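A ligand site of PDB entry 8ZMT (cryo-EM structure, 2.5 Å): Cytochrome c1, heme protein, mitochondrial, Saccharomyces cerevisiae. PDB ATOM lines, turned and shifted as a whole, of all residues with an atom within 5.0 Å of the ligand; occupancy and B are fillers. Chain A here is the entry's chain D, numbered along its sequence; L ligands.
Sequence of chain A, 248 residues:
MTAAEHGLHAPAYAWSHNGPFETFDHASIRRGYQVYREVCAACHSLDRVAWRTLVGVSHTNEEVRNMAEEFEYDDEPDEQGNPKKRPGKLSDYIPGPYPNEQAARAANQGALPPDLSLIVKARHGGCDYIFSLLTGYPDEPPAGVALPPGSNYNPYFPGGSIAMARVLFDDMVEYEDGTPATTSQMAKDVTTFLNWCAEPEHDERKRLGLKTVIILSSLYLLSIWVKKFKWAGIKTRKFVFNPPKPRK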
ATOM      1  N   VAL A  39       9.420 -33.113  -8.184  1.00  0.00           N
ATOM      2  CA  VAL A  39       8.720 -32.445  -7.092  1.00  0.00           C
ATOM      3  C   VAL A  39       9.601 -31.390  -6.423  1.00  0.00           C
ATOM      4  O   VAL A  39       9.200 -30.223  -6.309  1.00  0.00           O
ATOM      5  CB  VAL A  39       8.215 -33.468  -6.060  1.00  0.00           C
ATOM      6  CG1 VAL A  39       7.728 -32.776  -4.829  1.00  0.00           C
ATOM      7  CG2 VAL A  39       7.092 -34.305  -6.641  1.00  0.00           C
ATOM      8  N   CYS A  40      10.791 -31.778  -5.947  1.00  0.00           N
ATOM      9  CA  CYS A  40      11.570 -30.883  -5.100  1.00  0.00           C
ATOM     10  C   CYS A  40      12.257 -29.766  -5.870  1.00  0.00           C
ATOM     11  O   CYS A  40      12.426 -28.671  -5.333  1.00  0.00           O
ATOM     12  CB  CYS A  40      12.664 -31.624  -4.332  1.00  0.00           C
ATOM     13  SG  CYS A  40      12.308 -33.238  -3.658  1.00  0.00           S
ATOM     14  N   CYS A  43      11.949 -25.585  -6.362  1.00  0.00           N
ATOM     15  CA  CYS A  43      12.349 -24.550  -5.430  1.00  0.00           C
ATOM     16  C   CYS A  43      13.658 -24.809  -4.702  1.00  0.00           C
ATOM     17  O   CYS A  43      14.125 -23.923  -3.993  1.00  0.00           O
ATOM     18  CB  CYS A  43      11.245 -24.312  -4.398  1.00  0.00           C
ATOM     19  SG  CYS A  43       9.776 -23.615  -5.138  1.00  0.00           S
ATOM     20  N   HIS A  44      14.275 -25.980  -4.856  1.00  0.00           N
ATOM     21  CA  HIS A  44      15.481 -26.319  -4.136  1.00  0.00           C
ATOM     22  C   HIS A  44      16.636 -26.596  -5.088  1.00  0.00           C
ATOM     23  O   HIS A  44      16.461 -27.236  -6.124  1.00  0.00           O
ATOM     24  CB  HIS A  44      15.254 -27.526  -3.241  1.00  0.00           C
ATOM     25  CG  HIS A  44      14.609 -27.182  -1.951  1.00  0.00           C
ATOM     26  ND1 HIS A  44      15.318 -26.674  -0.884  1.00  0.00           N
ATOM     27  CD2 HIS A  44      13.318 -27.227  -1.560  1.00  0.00           C
ATOM     28  CE1 HIS A  44      14.491 -26.445   0.119  1.00  0.00           C
ATOM     29  NE2 HIS A  44      13.273 -26.768  -0.267  1.00  0.00           N
ATOM     30  N   ASN A 108       8.561 -16.995  -3.111  1.00  0.00           N
ATOM     31  CA  ASN A 108       8.186 -17.798  -1.959  1.00  0.00           C
ATOM     32  C   ASN A 108       7.696 -16.932  -0.808  1.00  0.00           C
ATOM     33  O   ASN A 108       7.801 -17.331   0.359  1.00  0.00           O
ATOM     34  CB  ASN A 108       9.345 -18.678  -1.497  1.00  0.00           C
ATOM     35  CG  ASN A 108       9.557 -19.872  -2.401  1.00  0.00           C
ATOM     36  OD1 ASN A 108       8.794 -20.838  -2.346  1.00  0.00           O
ATOM     37  ND2 ASN A 108      10.576 -19.816  -3.228  1.00  0.00           N
ATOM     38  N   ALA A 111      10.303 -15.953   2.022  1.00  0.00           N
ATOM     39  CA  ALA A 111      11.077 -17.012   2.638  1.00  0.00           C
ATOM     40  C   ALA A 111      12.080 -17.593   1.654  1.00  0.00           C
ATOM     41  O   ALA A 111      11.878 -17.576   0.439  1.00  0.00           O
ATOM     42  CB  ALA A 111      10.159 -18.128   3.150  1.00  0.00           C
ATOM     43  N   LEU A 112      13.180 -18.114   2.190  1.00  0.00           N
ATOM     44  CA  LEU A 112      14.263 -18.646   1.373  1.00  0.00           C
ATOM     45  C   LEU A 112      14.389 -20.148   1.601  1.00  0.00           C
ATOM     46  O   LEU A 112      14.794 -20.562   2.701  1.00  0.00           O
ATOM     47  CB  LEU A 112      15.578 -17.939   1.703  1.00  0.00           C
ATOM     48  CG  LEU A 112      16.847 -18.391   0.973  1.00  0.00           C
ATOM     49  CD1 LEU A 112      16.722 -18.155  -0.502  1.00  0.00           C
ATOM     50  CD2 LEU A 112      18.055 -17.662   1.524  1.00  0.00           C
ATOM     51  N   PRO A 113      14.057 -21.001   0.625  1.00  0.00           N
ATOM     52  CA  PRO A 113      14.274 -22.437   0.794  1.00  0.00           C
ATOM     53  C   PRO A 113      15.753 -22.780   0.721  1.00  0.00           C
ATOM     54  O   PRO A 113      16.468 -22.291  -0.157  1.00  0.00           O
ATOM     55  CB  PRO A 113      13.506 -23.048  -0.395  1.00  0.00           C
ATOM     56  CG  PRO A 113      13.348 -21.951  -1.355  1.00  0.00           C
ATOM     57  CD  PRO A 113      13.284 -20.686  -0.583  1.00  0.00           C
ATOM     58  N   PRO A 114      16.246 -23.605   1.634  1.00  0.00           N
ATOM     59  CA  PRO A 114      17.685 -23.842   1.723  1.00  0.00           C
ATOM     60  C   PRO A 114      18.194 -24.864   0.705  1.00  0.00           C
ATOM     61  O   PRO A 114      17.434 -25.562   0.033  1.00  0.00           O
ATOM     62  CB  PRO A 114      17.868 -24.385   3.149  1.00  0.00           C
ATOM     63  CG  PRO A 114      16.574 -24.987   3.483  1.00  0.00           C
ATOM     64  CD  PRO A 114      15.517 -24.202   2.773  1.00  0.00           C
ATOM     65  N   LEU A 116      19.795 -28.328  -0.256  1.00  0.00           N
ATOM     66  CA  LEU A 116      19.529 -29.633   0.321  1.00  0.00           C
ATOM     67  C   LEU A 116      20.704 -30.597   0.224  1.00  0.00           C
ATOM     68  O   LEU A 116      20.507 -31.801   0.391  1.00  0.00           O
ATOM     69  CB  LEU A 116      18.296 -30.259  -0.336  1.00  0.00           C
ATOM     70  CG  LEU A 116      16.919 -29.664  -0.043  1.00  0.00           C
ATOM     71  CD1 LEU A 116      15.836 -30.531  -0.618  1.00  0.00           C
ATOM     72  CD2 LEU A 116      16.705 -29.455   1.438  1.00  0.00           C
ATOM     73  N   ILE A 119      21.486 -31.295   4.187  1.00  0.00           N
ATOM     74  CA  ILE A 119      20.389 -31.047   5.112  1.00  0.00           C
ATOM     75  C   ILE A 119      20.195 -32.193   6.105  1.00  0.00           C
ATOM     76  O   ILE A 119      19.564 -32.005   7.146  1.00  0.00           O
ATOM     77  CB  ILE A 119      19.093 -30.760   4.309  1.00  0.00           C
ATOM     78  CG1 ILE A 119      18.089 -29.955   5.128  1.00  0.00           C
ATOM     79  CG2 ILE A 119      18.449 -32.028   3.810  1.00  0.00           C
ATOM     80  CD1 ILE A 119      18.512 -28.551   5.390  1.00  0.00           C
ATOM     81  N   ARG A 123      20.672 -31.062  10.625  1.00  0.00           N
ATOM     82  CA  ARG A 123      19.492 -31.013  11.484  1.00  0.00           C
ATOM     83  C   ARG A 123      19.628 -32.062  12.563  1.00  0.00           C
ATOM     84  O   ARG A 123      20.112 -33.170  12.318  1.00  0.00           O
ATOM     85  CB  ARG A 123      18.207 -31.244  10.686  1.00  0.00           C
ATOM     86  CG  ARG A 123      17.815 -30.130   9.759  1.00  0.00           C
ATOM     87  CD  ARG A 123      17.651 -28.809  10.494  1.00  0.00           C
ATOM     88  NE  ARG A 123      17.225 -27.737   9.597  1.00  0.00           N
ATOM     89  CZ  ARG A 123      18.053 -26.982   8.891  1.00  0.00           C
ATOM     90  NH1 ARG A 123      17.576 -26.027   8.109  1.00  0.00           N
ATOM     91  NH2 ARG A 123      19.364 -27.173   8.965  1.00  0.00           N
ATOM     92  N   TYR A 129      14.070 -36.966  11.127  1.00  0.00           N
ATOM     93  CA  TYR A 129      13.444 -35.650  11.179  1.00  0.00           C
ATOM     94  C   TYR A 129      12.852 -35.270   9.820  1.00  0.00           C
ATOM     95  O   TYR A 129      11.772 -34.688   9.752  1.00  0.00           O
ATOM     96  CB  TYR A 129      14.454 -34.592  11.631  1.00  0.00           C
ATOM     97  CG  TYR A 129      13.964 -33.175  11.459  1.00  0.00           C
ATOM     98  CD1 TYR A 129      12.924 -32.690  12.242  1.00  0.00           C
ATOM     99  CD2 TYR A 129      14.517 -32.338  10.502  1.00  0.00           C
ATOM    100  CE1 TYR A 129      12.466 -31.401  12.084  1.00  0.00           C
ATOM    101  CE2 TYR A 129      14.056 -31.052  10.330  1.00  0.00           C
ATOM    102  CZ  TYR A 129      13.034 -30.590  11.129  1.00  0.00           C
ATOM    103  OH  TYR A 129      12.574 -29.314  10.967  1.00  0.00           O
ATOM    104  N   ILE A 130      13.561 -35.606   8.737  1.00  0.00           N
ATOM    105  CA  ILE A 130      13.094 -35.242   7.395  1.00  0.00           C
ATOM    106  C   ILE A 130      11.871 -36.059   7.011  1.00  0.00           C
ATOM    107  O   ILE A 130      10.959 -35.554   6.340  1.00  0.00           O
ATOM    108  CB  ILE A 130      14.240 -35.430   6.374  1.00  0.00           C
ATOM    109  CG1 ILE A 130      15.558 -34.887   6.923  1.00  0.00           C
ATOM    110  CG2 ILE A 130      13.889 -34.780   5.045  1.00  0.00           C
ATOM    111  CD1 ILE A 130      15.677 -33.391   6.935  1.00  0.00           C
ATOM    112  N   LEU A 133       8.791 -34.741   9.008  1.00  0.00           N
ATOM    113  CA  LEU A 133       8.331 -33.428   8.580  1.00  0.00           C
ATOM    114  C   LEU A 133       7.422 -33.531   7.361  1.00  0.00           C
ATOM    115  O   LEU A 133       6.369 -32.884   7.311  1.00  0.00           O
ATOM    116  CB  LEU A 133       9.525 -32.525   8.289  1.00  0.00           C
ATOM    117  CG  LEU A 133       9.255 -31.040   8.061  1.00  0.00           C
ATOM    118  CD1 LEU A 133       8.871 -30.359   9.348  1.00  0.00           C
ATOM    119  CD2 LEU A 133      10.474 -30.381   7.457  1.00  0.00           C
ATOM    120  N   LEU A 134       7.804 -34.353   6.384  1.00  0.00           N
ATOM    121  CA  LEU A 134       7.064 -34.442   5.138  1.00  0.00           C
ATOM    122  C   LEU A 134       5.747 -35.191   5.280  1.00  0.00           C
ATOM    123  O   LEU A 134       4.855 -35.004   4.445  1.00  0.00           O
ATOM    124  CB  LEU A 134       7.915 -35.118   4.071  1.00  0.00           C
ATOM    125  CG  LEU A 134       9.216 -34.428   3.695  1.00  0.00           C
ATOM    126  CD1 LEU A 134      10.075 -35.375   2.897  1.00  0.00           C
ATOM    127  CD2 LEU A 134       8.925 -33.171   2.909  1.00  0.00           C
ATOM    128  N   PHE A 157       8.313 -28.850  13.381  1.00  0.00           N
ATOM    129  CA  PHE A 157       9.088 -27.635  13.146  1.00  0.00           C
ATOM    130  C   PHE A 157       9.122 -26.803  14.426  1.00  0.00           C
ATOM    131  O   PHE A 157       8.094 -26.691  15.102  1.00  0.00           O
ATOM    132  CB  PHE A 157       8.470 -26.824  12.024  1.00  0.00           C
ATOM    133  CG  PHE A 157       9.394 -25.788  11.454  1.00  0.00           C
ATOM    134  CD1 PHE A 157      10.570 -26.145  10.846  1.00  0.00           C
ATOM    135  CD2 PHE A 157       9.063 -24.449  11.534  1.00  0.00           C
ATOM    136  CE1 PHE A 157      11.413 -25.187  10.323  1.00  0.00           C
ATOM    137  CE2 PHE A 157       9.906 -23.491  11.010  1.00  0.00           C
ATOM    138  CZ  PHE A 157      11.076 -23.865  10.414  1.00  0.00           C
ATOM    139  N   SER A 161       5.274 -23.247  12.982  1.00  0.00           N
ATOM    140  CA  SER A 161       4.826 -22.429  11.856  1.00  0.00           C
ATOM    141  C   SER A 161       5.895 -22.453  10.779  1.00  0.00           C
ATOM    142  O   SER A 161       6.995 -21.927  10.975  1.00  0.00           O
ATOM    143  CB  SER A 161       4.529 -20.999  12.299  1.00  0.00           C
ATOM    144  OG  SER A 161       4.139 -20.201  11.211  1.00  0.00           O
ATOM    145  N   ILE A 162       5.577 -23.055   9.636  1.00  0.00           N
ATOM    146  CA  ILE A 162       6.540 -23.273   8.561  1.00  0.00           C
ATOM    147  C   ILE A 162       6.006 -22.614   7.286  1.00  0.00           C
ATOM    148  O   ILE A 162       4.794 -22.478   7.103  1.00  0.00           O
ATOM    149  CB  ILE A 162       6.815 -24.790   8.383  1.00  0.00           C
ATOM    150  CG1 ILE A 162       8.079 -25.036   7.543  1.00  0.00           C
ATOM    151  CG2 ILE A 162       5.601 -25.538   7.843  1.00  0.00           C
ATOM    152  CD1 ILE A 162       8.505 -26.461   7.479  1.00  0.00           C
ATOM    153  N   ALA A 163       6.928 -22.164   6.437  1.00  0.00           N
ATOM    154  CA  ALA A 163       6.578 -21.483   5.197  1.00  0.00           C
ATOM    155  C   ALA A 163       6.477 -22.419   3.996  1.00  0.00           C
ATOM    156  O   ALA A 163       6.311 -21.938   2.881  1.00  0.00           O
ATOM    157  CB  ALA A 163       7.596 -20.382   4.904  1.00  0.00           C
ATOM    158  N   MET A 164       6.579 -23.718   4.209  1.00  0.00           N
ATOM    159  CA  MET A 164       6.398 -24.731   3.171  1.00  0.00           C
ATOM    160  C   MET A 164       5.066 -25.444   3.375  1.00  0.00           C
ATOM    161  O   MET A 164       4.787 -25.929   4.471  1.00  0.00           O
ATOM    162  CB  MET A 164       7.549 -25.747   3.208  1.00  0.00           C
ATOM    163  CG  MET A 164       7.270 -27.003   2.424  1.00  0.00           C
ATOM    164  SD  MET A 164       8.564 -28.257   2.462  1.00  0.00           S
ATOM    165  CE  MET A 164       8.701 -28.649   4.196  1.00  0.00           C
ATOM    166  N   VAL A 167       3.292 -30.976   0.135  1.00  0.00           N
ATOM    167  CA  VAL A 167       3.639 -31.135  -1.279  1.00  0.00           C
ATOM    168  C   VAL A 167       3.326 -32.547  -1.758  1.00  0.00           C
ATOM    169  O   VAL A 167       2.931 -32.753  -2.911  1.00  0.00           O
ATOM    170  CB  VAL A 167       5.128 -30.796  -1.527  1.00  0.00           C
ATOM    171  CG1 VAL A 167       5.386 -30.686  -2.996  1.00  0.00           C
ATOM    172  CG2 VAL A 167       5.522 -29.510  -0.845  1.00  0.00           C
ATOM    173  N   LEU A 168       3.464 -33.536  -0.876  1.00  0.00           N
ATOM    174  CA  LEU A 168       3.384 -34.934  -1.269  1.00  0.00           C
ATOM    175  C   LEU A 168       1.946 -35.430  -1.188  1.00  0.00           C
ATOM    176  O   LEU A 168       1.324 -35.376  -0.127  1.00  0.00           O
ATOM    177  CB  LEU A 168       4.285 -35.800  -0.395  1.00  0.00           C
ATOM    178  CG  LEU A 168       5.787 -35.679  -0.621  1.00  0.00           C
ATOM    179  CD1 LEU A 168       6.533 -36.577   0.333  1.00  0.00           C
ATOM    180  CD2 LEU A 168       6.130 -36.032  -2.059  1.00  0.00           C
ATOM    181  N   VAL A 190      13.085 -40.055  -0.930  1.00  0.00           N
ATOM    182  CA  VAL A 190      13.860 -38.820  -0.963  1.00  0.00           C
ATOM    183  C   VAL A 190      14.841 -38.760   0.192  1.00  0.00           C
ATOM    184  O   VAL A 190      15.930 -38.198   0.059  1.00  0.00           O
ATOM    185  CB  VAL A 190      12.945 -37.575  -0.982  1.00  0.00           C
ATOM    186  CG1 VAL A 190      12.333 -37.396  -2.309  1.00  0.00           C
ATOM    187  CG2 VAL A 190      11.865 -37.674   0.065  1.00  0.00           C
ATOM    188  N   LEU A 194      18.707 -38.234  -0.190  1.00  0.00           N
ATOM    189  CA  LEU A 194      19.334 -37.041   0.394  1.00  0.00           C
ATOM    190  C   LEU A 194      20.413 -37.417   1.389  1.00  0.00           C
ATOM    191  O   LEU A 194      21.332 -36.631   1.630  1.00  0.00           O
ATOM    192  CB  LEU A 194      18.282 -36.149   1.049  1.00  0.00           C
ATOM    193  CG  LEU A 194      17.462 -35.263   0.118  1.00  0.00           C
ATOM    194  CD1 LEU A 194      16.427 -34.483   0.912  1.00  0.00           C
ATOM    195  CD2 LEU A 194      18.348 -34.336  -0.686  1.00  0.00           C
HETATM  196  C1  LIG L   1      12.056 -25.834   3.732  1.00  0.00           C
HETATM  197  C2  LIG L   1      12.632 -30.278   1.907  1.00  0.00           C
HETATM  198  C3  LIG L   1       9.499 -29.188  -1.609  1.00  0.00           C
HETATM  199  C4  LIG L   1       9.589 -24.554  -0.229  1.00  0.00           C
HETATM  200  C5  LIG L   1      12.458 -27.141   3.567  1.00  0.00           C
HETATM  201  C6  LIG L   1      13.296 -27.884   4.486  1.00  0.00           C
HETATM  202  C7  LIG L   1      13.449 -29.111   3.983  1.00  0.00           C
HETATM  203  C8  LIG L   1      12.721 -29.196   2.741  1.00  0.00           C
HETATM  204  C9  LIG L   1      14.275 -30.262   4.609  1.00  0.00           C
HETATM  205  C10 LIG L   1      13.912 -27.337   5.783  1.00  0.00           C
HETATM  206  C11 LIG L   1      13.060 -27.595   7.019  1.00  0.00           C
HETATM  207  C12 LIG L   1      13.793 -27.027   8.194  1.00  0.00           C
HETATM  208  O1  LIG L   1      13.577 -27.492   9.340  1.00  0.00           O
HETATM  209  O2  LIG L   1      14.627 -26.116   7.998  1.00  0.00           O
HETATM  210  C13 LIG L   1      11.746 -30.391   0.855  1.00  0.00           C
HETATM  211  C14 LIG L   1      11.344 -31.620   0.237  1.00  0.00           C
HETATM  212  C15 LIG L   1      10.476 -31.312  -0.761  1.00  0.00           C
HETATM  213  C16 LIG L   1      10.300 -29.884  -0.752  1.00  0.00           C
HETATM  214  C17 LIG L   1      11.922 -32.981   0.689  1.00  0.00           C
HETATM  215  C18 LIG L   1       9.669 -32.196  -1.752  1.00  0.00           C
HETATM  216  C19 LIG L   1       9.436 -33.509  -1.672  1.00  0.00           C
HETATM  217  C20 LIG L   1       9.253 -27.833  -1.549  1.00  0.00           C
HETATM  218  C21 LIG L   1       8.375 -27.096  -2.430  1.00  0.00           C
HETATM  219  C22 LIG L   1       8.408 -25.799  -2.051  1.00  0.00           C
HETATM  220  C23 LIG L   1       9.290 -25.704  -0.913  1.00  0.00           C
HETATM  221  C24 LIG L   1       7.612 -27.779  -3.583  1.00  0.00           C
HETATM  222  C25 LIG L   1       7.670 -24.531  -2.563  1.00  0.00           C
HETATM  223  C26 LIG L   1       6.727 -24.437  -3.509  1.00  0.00           C
HETATM  224  C27 LIG L   1      10.233 -24.492   0.982  1.00  0.00           C
HETATM  225  C28 LIG L   1      10.383 -23.314   1.814  1.00  0.00           C
HETATM  226  C29 LIG L   1      11.061 -23.675   2.902  1.00  0.00           C
HETATM  227  C30 LIG L   1      11.366 -25.080   2.805  1.00  0.00           C
HETATM  228  C31 LIG L   1       9.856 -21.906   1.496  1.00  0.00           C
HETATM  229  C32 LIG L   1      11.456 -22.750   4.072  1.00  0.00           C
HETATM  230  C33 LIG L   1      10.441 -22.971   5.191  1.00  0.00           C
HETATM  231  C34 LIG L   1      10.787 -22.105   6.383  1.00  0.00           C
HETATM  232  O3  LIG L   1      11.966 -21.726   6.537  1.00  0.00           O
HETATM  233  O4  LIG L   1       9.861 -21.804   7.177  1.00  0.00           O
HETATM  234  N1  LIG L   1      12.123 -27.964   2.518  1.00  0.00           N
HETATM  235  N2  LIG L   1      11.087 -29.348   0.236  1.00  0.00           N
HETATM  236  N3  LIG L   1       9.794 -26.961  -0.638  1.00  0.00           N
HETATM  237  N4  LIG L   1      10.841 -25.541   1.620  1.00  0.00           N
HETATM  238 FE1  LIG L   1      10.953 -27.435   0.928  1.00  0.00          FE
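OH of Tyr 129 is in hydrogen-bond range of O1 of the ligand (2.6 Å). NH1 of Arg 123 lies within salt-bridge range of O2 of the ligand, 3.0 Å away. N of Ala 163 sits at hydrogen-bond distance from O4 of the ligand.
A ring nitrogen (ND1) of His 44 lies within hydrogen-bond range of the backbone carbonyl oxygen (O) of Pro 114 (2.6 Å).
A nitrogen (N1) of the ligand lies close to a ring nitrogen (NE2) of His 44, 3.2 Å away. A nitrogen (N2) of the ligand sits close to the side-chain sulfur (SD) of Met 164 (3.5 Å). Merely in contact with the ligand: Val 39, Cys 40, Cys 43, Asn 108, Pro 113, Pro 114, Ile 119, Leu 133, Leu 134, Phe 157, Ile 162 and Val 167. Hydrophobic or aromatic side chains within 4 Å of the ligand: Val 39, His 44, Pro 113, Pro 114, Ile 119, Tyr 129, Leu 133, Leu 134, Phe 157, Ile 162, Ala 163, Met 164 and Val 167. 17 residues have an atom within 4 Å of the ligand: Val 39, Cys 40, Cys 43, His 44, Asn 108, Pro 113, Pro 114, Ile 119, Arg 123, Tyr 129, Leu 133, Leu 134, Phe 157, Ile 162, Ala 163, Met 164 and Val 167. Along chain A the residues within 4 Å of the ligand span positions 39 to 167.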
